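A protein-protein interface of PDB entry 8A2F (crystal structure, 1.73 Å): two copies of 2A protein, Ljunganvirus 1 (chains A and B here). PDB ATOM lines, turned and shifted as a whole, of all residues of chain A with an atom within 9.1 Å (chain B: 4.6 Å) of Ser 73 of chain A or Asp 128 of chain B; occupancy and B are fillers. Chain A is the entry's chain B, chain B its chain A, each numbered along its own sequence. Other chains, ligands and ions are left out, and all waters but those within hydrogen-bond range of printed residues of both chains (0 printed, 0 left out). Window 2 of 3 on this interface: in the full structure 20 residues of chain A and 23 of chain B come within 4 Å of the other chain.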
ATOM      1  N   THR A  67      -2.960  -4.079   5.176  1.00  0.00           N
ATOM      2  CA  THR A  67      -3.225  -4.414   3.783  1.00  0.00           C
ATOM      3  C   THR A  67      -3.620  -5.882   3.658  1.00  0.00           C
ATOM      4  O   THR A  67      -4.502  -6.213   2.867  1.00  0.00           O
ATOM      5  CB  THR A  67      -2.053  -4.062   2.855  1.00  0.00           C
ATOM      6  OG1 THR A  67      -0.891  -4.812   3.219  1.00  0.00           O
ATOM      7  CG2 THR A  67      -1.703  -2.593   2.892  1.00  0.00           C
ATOM      8  N   GLU A  68      -2.967  -6.764   4.433  1.00  0.00           N
ATOM      9  CA  GLU A  68      -3.328  -8.173   4.433  1.00  0.00           C
ATOM     10  C   GLU A  68      -4.772  -8.337   4.899  1.00  0.00           C
ATOM     11  O   GLU A  68      -5.509  -9.154   4.357  1.00  0.00           O
ATOM     12  CB  GLU A  68      -2.376  -8.968   5.332  1.00  0.00           C
ATOM     13  CG  GLU A  68      -2.748 -10.424   5.507  1.00  0.00           C
ATOM     14  CD  GLU A  68      -2.447 -11.324   4.322  1.00  0.00           C
ATOM     15  OE1 GLU A  68      -2.180 -10.804   3.217  1.00  0.00           O
ATOM     16  OE2 GLU A  68      -2.452 -12.556   4.520  1.00  0.00           O
ATOM     17  N   LYS A  69      -5.171  -7.555   5.901  1.00  0.00           N
ATOM     18  CA  LYS A  69      -6.484  -7.711   6.503  1.00  0.00           C
ATOM     19  C   LYS A  69      -7.579  -7.161   5.589  1.00  0.00           C
ATOM     20  O   LYS A  69      -8.622  -7.784   5.453  1.00  0.00           O
ATOM     21  CB  LYS A  69      -6.490  -7.028   7.870  1.00  0.00           C
ATOM     22  CG  LYS A  69      -7.662  -7.376   8.773  1.00  0.00           C
ATOM     23  CD  LYS A  69      -7.287  -7.231  10.237  1.00  0.00           C
ATOM     24  CE  LYS A  69      -8.471  -7.042  11.159  1.00  0.00           C
ATOM     25  NZ  LYS A  69      -9.290  -8.270  11.305  1.00  0.00           N
ATOM     26  N   TYR A  70      -7.338  -6.012   4.945  1.00  0.00           N
ATOM     27  CA  TYR A  70      -8.409  -5.256   4.288  1.00  0.00           C
ATOM     28  C   TYR A  70      -8.268  -5.100   2.775  1.00  0.00           C
ATOM     29  O   TYR A  70      -9.240  -4.698   2.126  1.00  0.00           O
ATOM     30  CB  TYR A  70      -8.479  -3.846   4.873  1.00  0.00           C
ATOM     31  CG  TYR A  70      -8.844  -3.796   6.332  1.00  0.00           C
ATOM     32  CD1 TYR A  70      -9.979  -4.425   6.824  1.00  0.00           C
ATOM     33  CD2 TYR A  70      -8.064  -3.073   7.218  1.00  0.00           C
ATOM     34  CE1 TYR A  70     -10.289  -4.387   8.174  1.00  0.00           C
ATOM     35  CE2 TYR A  70      -8.368  -3.013   8.567  1.00  0.00           C
ATOM     36  CZ  TYR A  70      -9.499  -3.655   9.041  1.00  0.00           C
ATOM     37  OH  TYR A  70      -9.785  -3.573  10.382  1.00  0.00           O
ATOM     38  N   ILE A  71      -7.065  -5.290   2.217  1.00  0.00           N
ATOM     39  CA  ILE A  71      -6.844  -5.107   0.789  1.00  0.00           C
ATOM     40  C   ILE A  71      -6.671  -6.516   0.227  1.00  0.00           C
ATOM     41  O   ILE A  71      -5.573  -6.941  -0.109  1.00  0.00           O
ATOM     42  CB  ILE A  71      -5.618  -4.215   0.477  1.00  0.00           C
ATOM     43  CG1 ILE A  71      -5.676  -2.833   1.138  1.00  0.00           C
ATOM     44  CG2 ILE A  71      -5.424  -4.085  -1.029  1.00  0.00           C
ATOM     45  CD1 ILE A  71      -6.537  -1.821   0.405  1.00  0.00           C
ATOM     46  N   ASN A  72      -7.759  -7.278   0.235  1.00  0.00           N
ATOM     47  CA  ASN A  72      -7.680  -8.722   0.065  1.00  0.00           C
ATOM     48  C   ASN A  72      -7.951  -9.074  -1.391  1.00  0.00           C
ATOM     49  O   ASN A  72      -8.499 -10.136  -1.696  1.00  0.00           O
ATOM     50  CB  ASN A  72      -8.627  -9.433   1.033  1.00  0.00           C
ATOM     51  CG  ASN A  72     -10.013  -8.826   1.071  1.00  0.00           C
ATOM     52  OD1 ASN A  72     -10.777  -8.943   0.115  1.00  0.00           O
ATOM     53  ND2 ASN A  72     -10.343  -8.170   2.170  1.00  0.00           N
ATOM     54  N   SER A  73      -7.539  -8.173  -2.286  1.00  0.00           N
ATOM     55  CA  SER A  73      -7.943  -8.226  -3.680  1.00  0.00           C
ATOM     56  C   SER A  73      -6.961  -7.420  -4.528  1.00  0.00           C
ATOM     57  O   SER A  73      -6.760  -6.228  -4.291  1.00  0.00           O
ATOM     58  CB  SER A  73      -9.368  -7.737  -3.818  1.00  0.00           C
ATOM     59  OG  SER A  73      -9.736  -7.597  -5.180  1.00  0.00           O
ATOM     60  N   MET A  74      -6.330  -8.099  -5.498  1.00  0.00           N
ATOM     61  CA  MET A  74      -5.479  -7.445  -6.478  1.00  0.00           C
ATOM     62  C   MET A  74      -6.337  -6.842  -7.595  1.00  0.00           C
ATOM     63  O   MET A  74      -5.797  -6.364  -8.592  1.00  0.00           O
ATOM     64  CB  MET A  74      -4.472  -8.435  -7.076  1.00  0.00           C
ATOM     65  N   VAL A  75      -7.670  -6.886  -7.424  1.00  0.00           N
ATOM     66  CA  VAL A  75      -8.616  -6.190  -8.284  1.00  0.00           C
ATOM     67  C   VAL A  75      -8.969  -4.845  -7.650  1.00  0.00           C
ATOM     68  O   VAL A  75      -9.007  -3.820  -8.325  1.00  0.00           O
ATOM     69  CB  VAL A  75      -9.882  -7.036  -8.530  1.00  0.00           C
ATOM     70  CG1 VAL A  75     -11.020  -6.203  -9.100  1.00  0.00           C
ATOM     71  CG2 VAL A  75      -9.596  -8.236  -9.424  1.00  0.00           C
ATOM     72  N   GLY A  76      -9.281  -4.868  -6.353  1.00  0.00           N
ATOM     73  CA  GLY A  76      -9.406  -3.643  -5.587  1.00  0.00           C
ATOM     74  C   GLY A  76     -10.818  -3.056  -5.626  1.00  0.00           C
ATOM     75  O   GLY A  76     -11.765  -3.661  -6.109  1.00  0.00           O
ATOM     76  N   SER A  77     -10.920  -1.826  -5.137  1.00  0.00           N
ATOM     77  CA  SER A  77     -12.173  -1.259  -4.678  1.00  0.00           C
ATOM     78  C   SER A  77     -12.934  -0.600  -5.820  1.00  0.00           C
ATOM     79  O   SER A  77     -12.328  -0.178  -6.805  1.00  0.00           O
ATOM     80  CB  SER A  77     -11.852  -0.259  -3.594  1.00  0.00           C
ATOM     81  OG  SER A  77     -13.031   0.197  -2.955  1.00  0.00           O
ATOM     82  N   LYS A  78     -14.256  -0.441  -5.657  1.00  0.00           N
ATOM     83  CA  LYS A  78     -15.034   0.383  -6.568  1.00  0.00           C
ATOM     84  C   LYS A  78     -14.991   1.854  -6.136  1.00  0.00           C
ATOM     85  O   LYS A  78     -15.447   2.734  -6.867  1.00  0.00           O
ATOM     86  CB  LYS A  78     -16.484  -0.104  -6.597  1.00  0.00           C
ATOM     87  CG  LYS A  78     -17.295   0.259  -5.360  1.00  0.00           C
ATOM     88  CD  LYS A  78     -18.735  -0.179  -5.436  1.00  0.00           C
ATOM     89  CE  LYS A  78     -19.554   0.267  -4.246  1.00  0.00           C
ATOM     90  NZ  LYS A  78     -20.327   1.509  -4.495  1.00  0.00           N
ATOM     91  N   LYS A 105      -2.295   5.178  -5.918  1.00  0.00           N
ATOM     92  CA  LYS A 105      -2.255   3.881  -5.264  1.00  0.00           C
ATOM     93  C   LYS A 105      -2.346   4.062  -3.749  1.00  0.00           C
ATOM     94  O   LYS A 105      -3.066   3.323  -3.079  1.00  0.00           O
ATOM     95  CB  LYS A 105      -0.955   3.158  -5.636  1.00  0.00           C
ATOM     96  CG  LYS A 105      -0.826   1.717  -5.171  1.00  0.00           C
ATOM     97  CD  LYS A 105      -1.711   0.753  -5.923  1.00  0.00           C
ATOM     98  CE  LYS A 105      -1.234  -0.683  -5.826  1.00  0.00           C
ATOM     99  NZ  LYS A 105      -1.881  -1.542  -6.844  1.00  0.00           N
ATOM    100  N   ILE A 109      -5.217   2.566  -1.139  1.00  0.00           N
ATOM    101  CA  ILE A 109      -4.897   1.622  -0.082  1.00  0.00           C
ATOM    102  C   ILE A 109      -5.332   2.188   1.274  1.00  0.00           C
ATOM    103  O   ILE A 109      -6.037   1.534   2.037  1.00  0.00           O
ATOM    104  CB  ILE A 109      -3.412   1.244  -0.133  1.00  0.00           C
ATOM    105  CG1 ILE A 109      -3.084   0.446  -1.397  1.00  0.00           C
ATOM    106  CG2 ILE A 109      -2.999   0.495   1.124  1.00  0.00           C
ATOM    107  CD1 ILE A 109      -1.592   0.321  -1.653  1.00  0.00           C
ATOM    108  N   VAL A 112      -9.245   2.542   1.563  1.00  0.00           N
ATOM    109  CA  VAL A 112      -9.999   1.323   1.811  1.00  0.00           C
ATOM    110  C   VAL A 112      -9.771   0.852   3.242  1.00  0.00           C
ATOM    111  O   VAL A 112     -10.703   0.353   3.878  1.00  0.00           O
ATOM    112  CB  VAL A 112      -9.675   0.225   0.779  1.00  0.00           C
ATOM    113  CG1 VAL A 112     -10.229  -1.132   1.191  1.00  0.00           C
ATOM    114  CG2 VAL A 112     -10.186   0.625  -0.593  1.00  0.00           C
ATOM    115  N   LYS B  17     -22.769  -7.851  -1.334  1.00  0.00           N
ATOM    116  CA  LYS B  17     -23.033  -9.273  -1.414  1.00  0.00           C
ATOM    117  C   LYS B  17     -23.511  -9.777  -0.053  1.00  0.00           C
ATOM    118  O   LYS B  17     -22.940  -9.422   0.967  1.00  0.00           O
ATOM    119  CB  LYS B  17     -21.754 -10.022  -1.804  1.00  0.00           C
ATOM    120  CG  LYS B  17     -21.200  -9.684  -3.188  1.00  0.00           C
ATOM    121  CD  LYS B  17     -19.819 -10.270  -3.425  1.00  0.00           C
ATOM    122  CE  LYS B  17     -19.205  -9.887  -4.762  1.00  0.00           C
ATOM    123  NZ  LYS B  17     -18.372  -8.652  -4.646  1.00  0.00           N
ATOM    124  N   VAL B 125     -15.687  -4.141  -6.026  1.00  0.00           N
ATOM    125  CA  VAL B 125     -16.358  -4.185  -7.309  1.00  0.00           C
ATOM    126  C   VAL B 125     -17.287  -5.390  -7.247  1.00  0.00           C
ATOM    127  O   VAL B 125     -16.945  -6.408  -6.633  1.00  0.00           O
ATOM    128  CB  VAL B 125     -15.350  -4.246  -8.471  1.00  0.00           C
ATOM    129  CG1 VAL B 125     -14.458  -3.008  -8.488  1.00  0.00           C
ATOM    130  CG2 VAL B 125     -14.538  -5.521  -8.445  1.00  0.00           C
ATOM    131  N   PRO B 126     -18.513  -5.296  -7.798  1.00  0.00           N
ATOM    132  CA  PRO B 126     -19.580  -6.248  -7.486  1.00  0.00           C
ATOM    133  C   PRO B 126     -19.490  -7.595  -8.191  1.00  0.00           C
ATOM    134  O   PRO B 126     -20.222  -8.518  -7.857  1.00  0.00           O
ATOM    135  CB  PRO B 126     -20.819  -5.482  -7.926  1.00  0.00           C
ATOM    136  CG  PRO B 126     -20.327  -4.744  -9.125  1.00  0.00           C
ATOM    137  CD  PRO B 126     -19.005  -4.188  -8.631  1.00  0.00           C
ATOM    138  N   TRP B 127     -18.545  -7.716  -9.109  1.00  0.00           N
ATOM    139  CA  TRP B 127     -18.379  -8.948  -9.855  1.00  0.00           C
ATOM    140  C   TRP B 127     -17.234  -9.797  -9.320  1.00  0.00           C
ATOM    141  O   TRP B 127     -17.025 -10.913  -9.798  1.00  0.00           O
ATOM    142  CB  TRP B 127     -18.135  -8.614 -11.311  1.00  0.00           C
ATOM    143  CG  TRP B 127     -17.037  -7.621 -11.563  1.00  0.00           C
ATOM    144  CD1 TRP B 127     -17.190  -6.278 -11.764  1.00  0.00           C
ATOM    145  CD2 TRP B 127     -15.635  -7.893 -11.733  1.00  0.00           C
ATOM    146  NE1 TRP B 127     -15.987  -5.705 -12.065  1.00  0.00           N
ATOM    147  CE2 TRP B 127     -15.009  -6.658 -12.020  1.00  0.00           C
ATOM    148  CE3 TRP B 127     -14.842  -9.042 -11.646  1.00  0.00           C
ATOM    149  CZ2 TRP B 127     -13.637  -6.547 -12.233  1.00  0.00           C
ATOM    150  CZ3 TRP B 127     -13.488  -8.931 -11.864  1.00  0.00           C
ATOM    151  CH2 TRP B 127     -12.896  -7.704 -12.148  1.00  0.00           C
ATOM    152  N   ASP B 128     -16.457  -9.240  -8.394  1.00  0.00           N
ATOM    153  CA  ASP B 128     -15.259  -9.910  -7.915  1.00  0.00           C
ATOM    154  C   ASP B 128     -15.701 -10.917  -6.846  1.00  0.00           C
ATOM    155  O   ASP B 128     -15.839 -10.557  -5.678  1.00  0.00           O
ATOM    156  CB  ASP B 128     -14.252  -8.845  -7.459  1.00  0.00           C
ATOM    157  CG  ASP B 128     -12.900  -9.352  -6.985  1.00  0.00           C
ATOM    158  OD1 ASP B 128     -12.561 -10.520  -7.290  1.00  0.00           O
ATOM    159  OD2 ASP B 128     -12.199  -8.566  -6.302  1.00  0.00           O
ATOM    160  N   TYR B 129     -15.953 -12.166  -7.274  1.00  0.00           N
ATOM    161  CA  TYR B 129     -16.488 -13.219  -6.413  1.00  0.00           C
ATOM    162  C   TYR B 129     -15.501 -13.573  -5.302  1.00  0.00           C
ATOM    163  O   TYR B 129     -15.913 -13.872  -4.180  1.00  0.00           O
ATOM    164  CB  TYR B 129     -16.817 -14.480  -7.222  1.00  0.00           C
ATOM    165  N   SER B 130     -14.202 -13.542  -5.637  1.00  0.00           N
ATOM    166  CA  SER B 130     -13.132 -13.919  -4.725  1.00  0.00           C
ATOM    167  C   SER B 130     -12.597 -12.691  -3.987  1.00  0.00           C
ATOM    168  O   SER B 130     -11.387 -12.563  -3.800  1.00  0.00           O
ATOM    169  CB  SER B 130     -12.024 -14.620  -5.478  1.00  0.00           C
ATOM    170  OG  SER B 130     -12.540 -15.642  -6.320  1.00  0.00           O
ATOM    171  N   SER B 131     -13.506 -11.810  -3.542  1.00  0.00           N
ATOM    172  CA  SER B 131     -13.136 -10.540  -2.936  1.00  0.00           C
ATOM    173  C   SER B 131     -13.073 -10.663  -1.411  1.00  0.00           C
ATOM    174  O   SER B 131     -13.574  -9.796  -0.704  1.00  0.00           O
ATOM    175  CB  SER B 131     -14.082  -9.430  -3.374  1.00  0.00           C
ATOM    176  OG  SER B 131     -15.449  -9.755  -3.117  1.00  0.00           O
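The side-chain hydroxyl (OG) of Ser 73 of chain A is in hydrogen-bond range of the side-chain carboxylate (OD2) of Asp 128 of chain B.
The side-chain amide oxygen (OD1) of Asn 72 of chain A sits close to the backbone carbonyl oxygen (O) of Ser 131 of chain B, 3.0 Å away.
The side-chain amino group of Lys 17 of chain B sits at hydrogen-bond distance from the backbone carbonyl oxygen of Val 125 of chain B (3.3 Å).
The side-chain amino group of Lys 17 of chain B is in hydrogen-bond range of the backbone carbonyl oxygen of Asp 128 of chain B, 3.3 Å away.
The side-chain amino group of Lys 17 of chain B lies within hydrogen-bond range of the side-chain hydroxyl of Ser 131 of chain B (3.5 Å).
The side-chain hydroxyl (OG) of Ser 131 of chain B lies within hydrogen-bond range of the backbone carbonyl oxygen (O) of Asp 128 of chain B (2.7 Å).
N of Val 75 of chain A sits close to OG of Ser 73 of chain A.
OG of Ser 73 of chain A is in hydrogen-bond range of N of Gly 76 of chain A (3.0 Å).
Val 125 of chain B touches Val 75 of chain A (CG2 to CG1, 3.6 Å).
Val 75 of chain A touches Trp 127 of chain B.
CB of Val 75 of chain A touches OD2 of Asp 128 of chain B (3.6 Å).
CG1 of Val 125 of chain B touches O of Gly 76 of chain A, at 3.7 Å.
Val 125 of chain B touches Ser 77 of chain A (CG1 to C, 3.9 Å).
N of Lys 78 of chain A touches CG1 of Val 125 of chain B (3.8 Å).
Ser 73 of chain A touches just one residue of chain B: Asp 128.
Met 74 of chain A touches none of the printed residues of chain B.
Of the printed residues of chain B, Val 75 of chain A touches Val 125 (3.6 Å), Trp 127 (3.9 Å) and Asp 128 (3.6 Å).
Lys 105 of chain A touches none of the printed residues of chain B.
Printed residues of chain A within 4 Å of Val 125 of chain B: Val 75, Gly 76, Ser 77 and Lys 78.
Of the printed residues of chain A, Trp 127 of chain B touches Val 75.
Asp 128 of chain B touches two residues of chain A.
No residue of chain A comes within 4 Å of Tyr 129 of chain B.
The nearest residue of chain A that does not touch Asp 128 of chain B is Gly 76 of chain A (4.7 Å).
Hydrophobic or aromatic side chains of chain B that line the printed part of chain A: Val 125 and Trp 127.
Along chain B the printed residues that touch a printed residue of chain A span positions 125 to 131.
Hydrophobic or aromatic side chains of chain A within 4 Å of the printed part of chain B: Val 75.
Among the printed residues, no Asp or Glu carboxylate lies within 4 Å of a Lys or Arg side-chain nitrogen of the other chain.
No position is printed for both chains.
Of the 8 pairs that touch across the chains among the printed residues, none has its exchanged pair printed and touching as well.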
